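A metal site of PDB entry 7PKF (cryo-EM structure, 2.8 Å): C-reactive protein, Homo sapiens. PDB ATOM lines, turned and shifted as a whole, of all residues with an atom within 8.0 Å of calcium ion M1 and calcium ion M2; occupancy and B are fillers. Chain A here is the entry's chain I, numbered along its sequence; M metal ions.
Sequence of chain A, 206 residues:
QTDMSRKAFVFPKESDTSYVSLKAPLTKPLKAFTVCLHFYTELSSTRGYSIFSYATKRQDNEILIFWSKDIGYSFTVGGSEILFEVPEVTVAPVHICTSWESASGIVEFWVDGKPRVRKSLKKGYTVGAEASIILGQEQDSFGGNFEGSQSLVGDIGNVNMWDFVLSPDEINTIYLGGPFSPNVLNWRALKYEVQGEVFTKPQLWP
O of Ser 53 lies within hydrogen-bond range of NE2 of Gln 139, 3.5 Å away. OE1 of Glu 138 is in hydrogen-bond range of OG of Ser 50 (3.0 Å). N of Asn 61 sits at hydrogen-bond distance from OE1 of Gln 59 (2.9 Å). N of Ala 55 sits close to NE2 of Gln 139 (3.2 Å). The backbone carbonyl oxygen of Gln 150 lies within hydrogen-bond range of the backbone NH of Ser 50 (2.8 Å).
Merely in contact with calcium ion M1: Gln 139. The nearest printed residue that does not touch calcium ion M1 is Leu 64 (4.8 Å).
Residues that only touch calcium ion M2: Glu 147 (3.3 Å). Four residues have an atom within 4 Å of calcium ion M2: Glu 138, Asp 140, Glu 147 and Gln 150.
Calcium ion M1 is bound by the side-chain carboxylate (OD2) of Asp 140 (2.3 Å), the side-chain amide oxygen (OD1) of Asn 61 (2.4 Å), the side-chain carboxylate (OE2) of Glu 138 (2.4 Å) and the side-chain carboxylate (OD2) of Asp 60 (2.7 Å).
Calcium ion M2 is bound by the side-chain carboxylate (OD1) of Asp 140 (2.4 Å) and the side-chain amide oxygen (OE1) of Gln 150 (2.5 Å). Slightly farther from calcium ion M2 lies OD2 of Asp 140 (3.0 Å).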
ATOM      1  N   SER A  50      -3.140 -15.090 -21.266  1.00  0.00           N
ATOM      2  CA  SER A  50      -3.136 -15.784 -19.982  1.00  0.00           C
ATOM      3  C   SER A  50      -1.730 -16.238 -19.580  1.00  0.00           C
ATOM      4  O   SER A  50      -1.083 -17.004 -20.309  1.00  0.00           O
ATOM      5  CB  SER A  50      -4.078 -16.978 -20.037  1.00  0.00           C
ATOM      6  OG  SER A  50      -4.145 -17.635 -18.778  1.00  0.00           O
ATOM      7  N   SER A  53      -3.884 -19.502 -15.308  1.00  0.00           N
ATOM      8  CA  SER A  53      -5.321 -19.654 -15.086  1.00  0.00           C
ATOM      9  C   SER A  53      -5.598 -20.789 -14.106  1.00  0.00           C
ATOM     10  O   SER A  53      -5.264 -21.948 -14.374  1.00  0.00           O
ATOM     11  CB  SER A  53      -6.046 -19.899 -16.400  1.00  0.00           C
ATOM     12  OG  SER A  53      -7.442 -19.944 -16.187  1.00  0.00           O
ATOM     13  N   TYR A  54      -6.213 -20.440 -12.979  1.00  0.00           N
ATOM     14  CA  TYR A  54      -6.684 -21.386 -11.973  1.00  0.00           C
ATOM     15  C   TYR A  54      -8.207 -21.292 -11.937  1.00  0.00           C
ATOM     16  O   TYR A  54      -8.756 -20.223 -11.671  1.00  0.00           O
ATOM     17  CB  TYR A  54      -6.070 -21.019 -10.632  1.00  0.00           C
ATOM     18  CG  TYR A  54      -6.355 -21.885  -9.421  1.00  0.00           C
ATOM     19  CD1 TYR A  54      -7.636 -22.001  -8.910  1.00  0.00           C
ATOM     20  CD2 TYR A  54      -5.322 -22.527  -8.761  1.00  0.00           C
ATOM     21  CE1 TYR A  54      -7.892 -22.749  -7.784  1.00  0.00           C
ATOM     22  CE2 TYR A  54      -5.570 -23.287  -7.637  1.00  0.00           C
ATOM     23  CZ  TYR A  54      -6.849 -23.390  -7.154  1.00  0.00           C
ATOM     24  OH  TYR A  54      -7.089 -24.153  -6.034  1.00  0.00           O
ATOM     25  N   ALA A  55      -8.877 -22.411 -12.193  1.00  0.00           N
ATOM     26  CA  ALA A  55     -10.339 -22.435 -12.309  1.00  0.00           C
ATOM     27  C   ALA A  55     -10.962 -23.523 -11.446  1.00  0.00           C
ATOM     28  O   ALA A  55     -10.312 -24.490 -11.044  1.00  0.00           O
ATOM     29  CB  ALA A  55     -10.797 -22.659 -13.753  1.00  0.00           C
ATOM     30  N   GLN A  59     -16.156 -21.309 -10.731  1.00  0.00           N
ATOM     31  CA  GLN A  59     -15.578 -20.042 -11.149  1.00  0.00           C
ATOM     32  C   GLN A  59     -14.346 -20.312 -12.000  1.00  0.00           C
ATOM     33  O   GLN A  59     -13.389 -20.923 -11.536  1.00  0.00           O
ATOM     34  CB  GLN A  59     -15.205 -19.183  -9.930  1.00  0.00           C
ATOM     35  CG  GLN A  59     -14.533 -17.865 -10.260  1.00  0.00           C
ATOM     36  CD  GLN A  59     -15.269 -17.075 -11.325  1.00  0.00           C
ATOM     37  OE1 GLN A  59     -14.927 -17.139 -12.506  1.00  0.00           O
ATOM     38  NE2 GLN A  59     -16.284 -16.339 -10.919  1.00  0.00           N
ATOM     39  N   ASP A  60     -14.378 -19.858 -13.256  1.00  0.00           N
ATOM     40  CA  ASP A  60     -13.320 -20.140 -14.216  1.00  0.00           C
ATOM     41  C   ASP A  60     -12.168 -19.148 -14.148  1.00  0.00           C
ATOM     42  O   ASP A  60     -11.170 -19.333 -14.847  1.00  0.00           O
ATOM     43  CB  ASP A  60     -13.893 -20.137 -15.639  1.00  0.00           C
ATOM     44  CG  ASP A  60     -14.196 -18.740 -16.133  1.00  0.00           C
ATOM     45  OD1 ASP A  60     -15.340 -18.268 -15.953  1.00  0.00           O
ATOM     46  OD2 ASP A  60     -13.297 -18.104 -16.715  1.00  0.00           O
ATOM     47  N   ASN A  61     -12.270 -18.117 -13.312  1.00  0.00           N
ATOM     48  CA  ASN A  61     -11.197 -17.168 -13.074  1.00  0.00           C
ATOM     49  C   ASN A  61     -10.885 -17.107 -11.586  1.00  0.00           C
ATOM     50  O   ASN A  61     -10.685 -16.035 -11.009  1.00  0.00           O
ATOM     51  CB  ASN A  61     -11.565 -15.779 -13.600  1.00  0.00           C
ATOM     52  CG  ASN A  61     -11.621 -15.723 -15.115  1.00  0.00           C
ATOM     53  OD1 ASN A  61     -11.063 -16.588 -15.798  1.00  0.00           O
ATOM     54  ND2 ASN A  61     -12.296 -14.714 -15.640  1.00  0.00           N
ATOM     55  N   GLU A  62     -10.842 -18.278 -10.942  1.00  0.00           N
ATOM     56  CA  GLU A  62     -10.696 -18.306  -9.495  1.00  0.00           C
ATOM     57  C   GLU A  62      -9.364 -17.719  -9.043  1.00  0.00           C
ATOM     58  O   GLU A  62      -9.320 -16.950  -8.076  1.00  0.00           O
ATOM     59  CB  GLU A  62     -10.838 -19.758  -9.019  1.00  0.00           C
ATOM     60  CG  GLU A  62     -10.627 -19.967  -7.538  1.00  0.00           C
ATOM     61  CD  GLU A  62     -11.851 -19.596  -6.735  1.00  0.00           C
ATOM     62  OE1 GLU A  62     -12.973 -19.752  -7.249  1.00  0.00           O
ATOM     63  OE2 GLU A  62     -11.695 -19.145  -5.595  1.00  0.00           O
ATOM     64  N   ILE A  63      -8.272 -18.069  -9.706  1.00  0.00           N
ATOM     65  CA  ILE A  63      -7.086 -17.219  -9.781  1.00  0.00           C
ATOM     66  C   ILE A  63      -6.723 -17.054 -11.251  1.00  0.00           C
ATOM     67  O   ILE A  63      -6.600 -18.045 -11.977  1.00  0.00           O
ATOM     68  CB  ILE A  63      -5.906 -17.803  -8.982  1.00  0.00           C
ATOM     69  CG1 ILE A  63      -6.291 -17.965  -7.513  1.00  0.00           C
ATOM     70  CG2 ILE A  63      -4.701 -16.896  -9.103  1.00  0.00           C
ATOM     71  CD1 ILE A  63      -5.364 -18.880  -6.730  1.00  0.00           C
ATOM     72  N   LEU A  64      -6.544 -15.807 -11.685  1.00  0.00           N
ATOM     73  CA  LEU A  64      -6.057 -15.530 -13.024  1.00  0.00           C
ATOM     74  C   LEU A  64      -4.962 -14.473 -12.948  1.00  0.00           C
ATOM     75  O   LEU A  64      -5.149 -13.412 -12.349  1.00  0.00           O
ATOM     76  CB  LEU A  64      -7.172 -15.071 -13.963  1.00  0.00           C
ATOM     77  CG  LEU A  64      -6.731 -14.769 -15.386  1.00  0.00           C
ATOM     78  CD1 LEU A  64      -6.141 -15.993 -16.053  1.00  0.00           C
ATOM     79  CD2 LEU A  64      -7.904 -14.253 -16.199  1.00  0.00           C
ATOM     80  N   PHE A  66      -3.094 -12.349 -15.793  1.00  0.00           N
ATOM     81  CA  PHE A  66      -3.339 -12.024 -17.184  1.00  0.00           C
ATOM     82  C   PHE A  66      -2.567 -10.761 -17.536  1.00  0.00           C
ATOM     83  O   PHE A  66      -2.491  -9.827 -16.747  1.00  0.00           O
ATOM     84  CB  PHE A  66      -4.844 -11.826 -17.434  1.00  0.00           C
ATOM     85  CG  PHE A  66      -5.242 -11.836 -18.872  1.00  0.00           C
ATOM     86  CD1 PHE A  66      -5.624 -13.015 -19.489  1.00  0.00           C
ATOM     87  CD2 PHE A  66      -5.286 -10.670 -19.607  1.00  0.00           C
ATOM     88  CE1 PHE A  66      -6.013 -13.027 -20.815  1.00  0.00           C
ATOM     89  CE2 PHE A  66      -5.660 -10.673 -20.932  1.00  0.00           C
ATOM     90  CZ  PHE A  66      -6.030 -11.862 -21.542  1.00  0.00           C
ATOM     91  N   THR A  76      -6.575 -11.462 -10.771  1.00  0.00           N
ATOM     92  CA  THR A  76      -7.946 -11.678 -10.330  1.00  0.00           C
ATOM     93  C   THR A  76      -8.013 -12.854  -9.368  1.00  0.00           C
ATOM     94  O   THR A  76      -7.336 -13.869  -9.553  1.00  0.00           O
ATOM     95  CB  THR A  76      -8.905 -11.991 -11.511  1.00  0.00           C
ATOM     96  OG1 THR A  76      -8.735 -13.283 -12.114  1.00  0.00           O
ATOM     97  CG2 THR A  76      -9.471 -10.824 -12.336  1.00  0.00           C
ATOM     98  N   GLN A 137      -3.240 -21.350 -21.876  1.00  0.00           N
ATOM     99  CA  GLN A 137      -4.568 -21.024 -22.343  1.00  0.00           C
ATOM    100  C   GLN A 137      -5.302 -20.263 -21.251  1.00  0.00           C
ATOM    101  O   GLN A 137      -4.920 -20.294 -20.075  1.00  0.00           O
ATOM    102  CB  GLN A 137      -5.371 -22.275 -22.732  1.00  0.00           C
ATOM    103  CG  GLN A 137      -4.774 -23.094 -23.853  1.00  0.00           C
ATOM    104  CD  GLN A 137      -4.754 -22.340 -25.173  1.00  0.00           C
ATOM    105  OE1 GLN A 137      -5.454 -21.350 -25.342  1.00  0.00           O
ATOM    106  NE2 GLN A 137      -3.943 -22.815 -26.107  1.00  0.00           N
ATOM    107  N   GLU A 138      -6.373 -19.579 -21.641  1.00  0.00           N
ATOM    108  CA  GLU A 138      -7.373 -19.096 -20.718  1.00  0.00           C
ATOM    109  C   GLU A 138      -8.608 -19.989 -20.782  1.00  0.00           C
ATOM    110  O   GLU A 138      -9.153 -20.218 -21.862  1.00  0.00           O
ATOM    111  CB  GLU A 138      -7.768 -17.652 -21.030  1.00  0.00           C
ATOM    112  CG  GLU A 138      -8.805 -17.070 -20.082  1.00  0.00           C
ATOM    113  CD  GLU A 138      -8.289 -16.955 -18.684  1.00  0.00           C
ATOM    114  OE1 GLU A 138      -7.058 -16.847 -18.525  1.00  0.00           O
ATOM    115  OE2 GLU A 138      -9.105 -16.984 -17.742  1.00  0.00           O
ATOM    116  N   GLN A 139      -9.039 -20.464 -19.622  1.00  0.00           N
ATOM    117  CA  GLN A 139     -10.099 -21.452 -19.510  1.00  0.00           C
ATOM    118  C   GLN A 139     -11.351 -20.796 -18.943  1.00  0.00           C
ATOM    119  O   GLN A 139     -11.296 -20.172 -17.884  1.00  0.00           O
ATOM    120  CB  GLN A 139      -9.632 -22.637 -18.660  1.00  0.00           C
ATOM    121  CG  GLN A 139      -9.394 -22.319 -17.203  1.00  0.00           C
ATOM    122  CD  GLN A 139      -8.783 -23.489 -16.471  1.00  0.00           C
ATOM    123  OE1 GLN A 139      -8.605 -24.551 -17.042  1.00  0.00           O
ATOM    124  NE2 GLN A 139      -8.371 -23.265 -15.234  1.00  0.00           N
ATOM    125  N   ASP A 140     -12.468 -20.948 -19.659  1.00  0.00           N
ATOM    126  CA  ASP A 140     -13.723 -20.313 -19.272  1.00  0.00           C
ATOM    127  C   ASP A 140     -14.803 -21.284 -18.861  1.00  0.00           C
ATOM    128  O   ASP A 140     -15.762 -20.875 -18.203  1.00  0.00           O
ATOM    129  CB  ASP A 140     -14.243 -19.453 -20.437  1.00  0.00           C
ATOM    130  CG  ASP A 140     -13.367 -18.247 -20.709  1.00  0.00           C
ATOM    131  OD1 ASP A 140     -13.534 -17.632 -21.781  1.00  0.00           O
ATOM    132  OD2 ASP A 140     -12.527 -17.911 -19.850  1.00  0.00           O
ATOM    133  N   SER A 141     -14.677 -22.568 -19.209  1.00  0.00           N
ATOM    134  CA  SER A 141     -15.266 -23.643 -18.426  1.00  0.00           C
ATOM    135  C   SER A 141     -14.241 -24.153 -17.426  1.00  0.00           C
ATOM    136  O   SER A 141     -13.151 -23.600 -17.273  1.00  0.00           O
ATOM    137  CB  SER A 141     -15.761 -24.765 -19.350  1.00  0.00           C
ATOM    138  OG  SER A 141     -14.698 -25.306 -20.111  1.00  0.00           O
ATOM    139  N   GLY A 144     -11.693 -25.724 -20.162  1.00  0.00           N
ATOM    140  CA  GLY A 144     -11.821 -25.613 -21.601  1.00  0.00           C
ATOM    141  C   GLY A 144     -12.430 -24.307 -22.045  1.00  0.00           C
ATOM    142  O   GLY A 144     -12.407 -23.312 -21.331  1.00  0.00           O
ATOM    143  N   ASN A 145     -12.971 -24.327 -23.273  1.00  0.00           N
ATOM    144  CA  ASN A 145     -13.463 -23.129 -23.949  1.00  0.00           C
ATOM    145  C   ASN A 145     -12.353 -22.090 -24.110  1.00  0.00           C
ATOM    146  O   ASN A 145     -12.567 -20.893 -23.930  1.00  0.00           O
ATOM    147  CB  ASN A 145     -14.669 -22.523 -23.236  1.00  0.00           C
ATOM    148  CG  ASN A 145     -15.818 -23.499 -23.099  1.00  0.00           C
ATOM    149  OD1 ASN A 145     -16.019 -24.365 -23.948  1.00  0.00           O
ATOM    150  ND2 ASN A 145     -16.598 -23.342 -22.039  1.00  0.00           N
ATOM    151  N   PHE A 146     -11.155 -22.561 -24.438  1.00  0.00           N
ATOM    152  CA  PHE A 146     -10.006 -21.669 -24.569  1.00  0.00           C
ATOM    153  C   PHE A 146     -10.224 -20.717 -25.747  1.00  0.00           C
ATOM    154  O   PHE A 146     -10.907 -21.039 -26.720  1.00  0.00           O
ATOM    155  CB  PHE A 146      -8.724 -22.468 -24.776  1.00  0.00           C
ATOM    156  CG  PHE A 146      -8.547 -23.597 -23.797  1.00  0.00           C
ATOM    157  CD1 PHE A 146      -8.537 -23.363 -22.440  1.00  0.00           C
ATOM    158  CD2 PHE A 146      -8.387 -24.897 -24.253  1.00  0.00           C
ATOM    159  CE1 PHE A 146      -8.372 -24.408 -21.540  1.00  0.00           C
ATOM    160  CE2 PHE A 146      -8.226 -25.943 -23.362  1.00  0.00           C
ATOM    161  CZ  PHE A 146      -8.213 -25.691 -22.010  1.00  0.00           C
ATOM    162  N   GLU A 147      -9.633 -19.533 -25.645  1.00  0.00           N
ATOM    163  CA  GLU A 147      -9.603 -18.566 -26.733  1.00  0.00           C
ATOM    164  C   GLU A 147      -8.178 -18.434 -27.246  1.00  0.00           C
ATOM    165  O   GLU A 147      -7.267 -18.103 -26.472  1.00  0.00           O
ATOM    166  CB  GLU A 147     -10.139 -17.211 -26.273  1.00  0.00           C
ATOM    167  CG  GLU A 147     -11.618 -17.231 -25.915  1.00  0.00           C
ATOM    168  CD  GLU A 147     -12.122 -15.873 -25.463  1.00  0.00           C
ATOM    169  OE1 GLU A 147     -11.310 -14.934 -25.344  1.00  0.00           O
ATOM    170  OE2 GLU A 147     -13.342 -15.740 -25.221  1.00  0.00           O
ATOM    171  N   GLY A 148      -7.987 -18.684 -28.538  1.00  0.00           N
ATOM    172  CA  GLY A 148      -6.661 -18.548 -29.136  1.00  0.00           C
ATOM    173  C   GLY A 148      -6.055 -17.171 -28.940  1.00  0.00           C
ATOM    174  O   GLY A 148      -4.861 -17.039 -28.683  1.00  0.00           O
ATOM    175  N   SER A 149      -6.877 -16.125 -29.063  1.00  0.00           N
ATOM    176  CA  SER A 149      -6.422 -14.756 -28.838  1.00  0.00           C
ATOM    177  C   SER A 149      -6.070 -14.461 -27.394  1.00  0.00           C
ATOM    178  O   SER A 149      -5.626 -13.345 -27.103  1.00  0.00           O
ATOM    179  CB  SER A 149      -7.505 -13.774 -29.302  1.00  0.00           C
ATOM    180  OG  SER A 149      -8.686 -13.916 -28.529  1.00  0.00           O
ATOM    181  N   GLN A 150      -6.268 -15.405 -26.472  1.00  0.00           N
ATOM    182  CA  GLN A 150      -5.787 -15.281 -25.103  1.00  0.00           C
ATOM    183  C   GLN A 150      -4.684 -16.278 -24.752  1.00  0.00           C
ATOM    184  O   GLN A 150      -4.207 -16.259 -23.604  1.00  0.00           O
ATOM    185  CB  GLN A 150      -6.962 -15.443 -24.143  1.00  0.00           C
ATOM    186  CG  GLN A 150      -7.988 -14.318 -24.260  1.00  0.00           C
ATOM    187  CD  GLN A 150      -8.912 -14.235 -23.070  1.00  0.00           C
ATOM    188  OE1 GLN A 150      -9.297 -15.257 -22.493  1.00  0.00           O
ATOM    189  NE2 GLN A 150      -9.269 -13.024 -22.672  1.00  0.00           N
ATOM    190  N   SER A 151      -4.256 -17.127 -25.679  1.00  0.00           N
ATOM    191  CA  SER A 151      -3.217 -18.105 -25.376  1.00  0.00           C
ATOM    192  C   SER A 151      -1.847 -17.455 -25.190  1.00  0.00           C
ATOM    193  O   SER A 151      -1.554 -16.389 -25.747  1.00  0.00           O
ATOM    194  CB  SER A 151      -3.141 -19.148 -26.487  1.00  0.00           C
ATOM    195  OG  SER A 151      -2.671 -18.578 -27.698  1.00  0.00           O
HETATM  196 CA    CA M   1     -11.488 -16.769 -18.130  1.00  0.00          CA
HETATM  197 CA    CA M   2     -11.414 -16.525 -22.268  1.00  0.00          CA
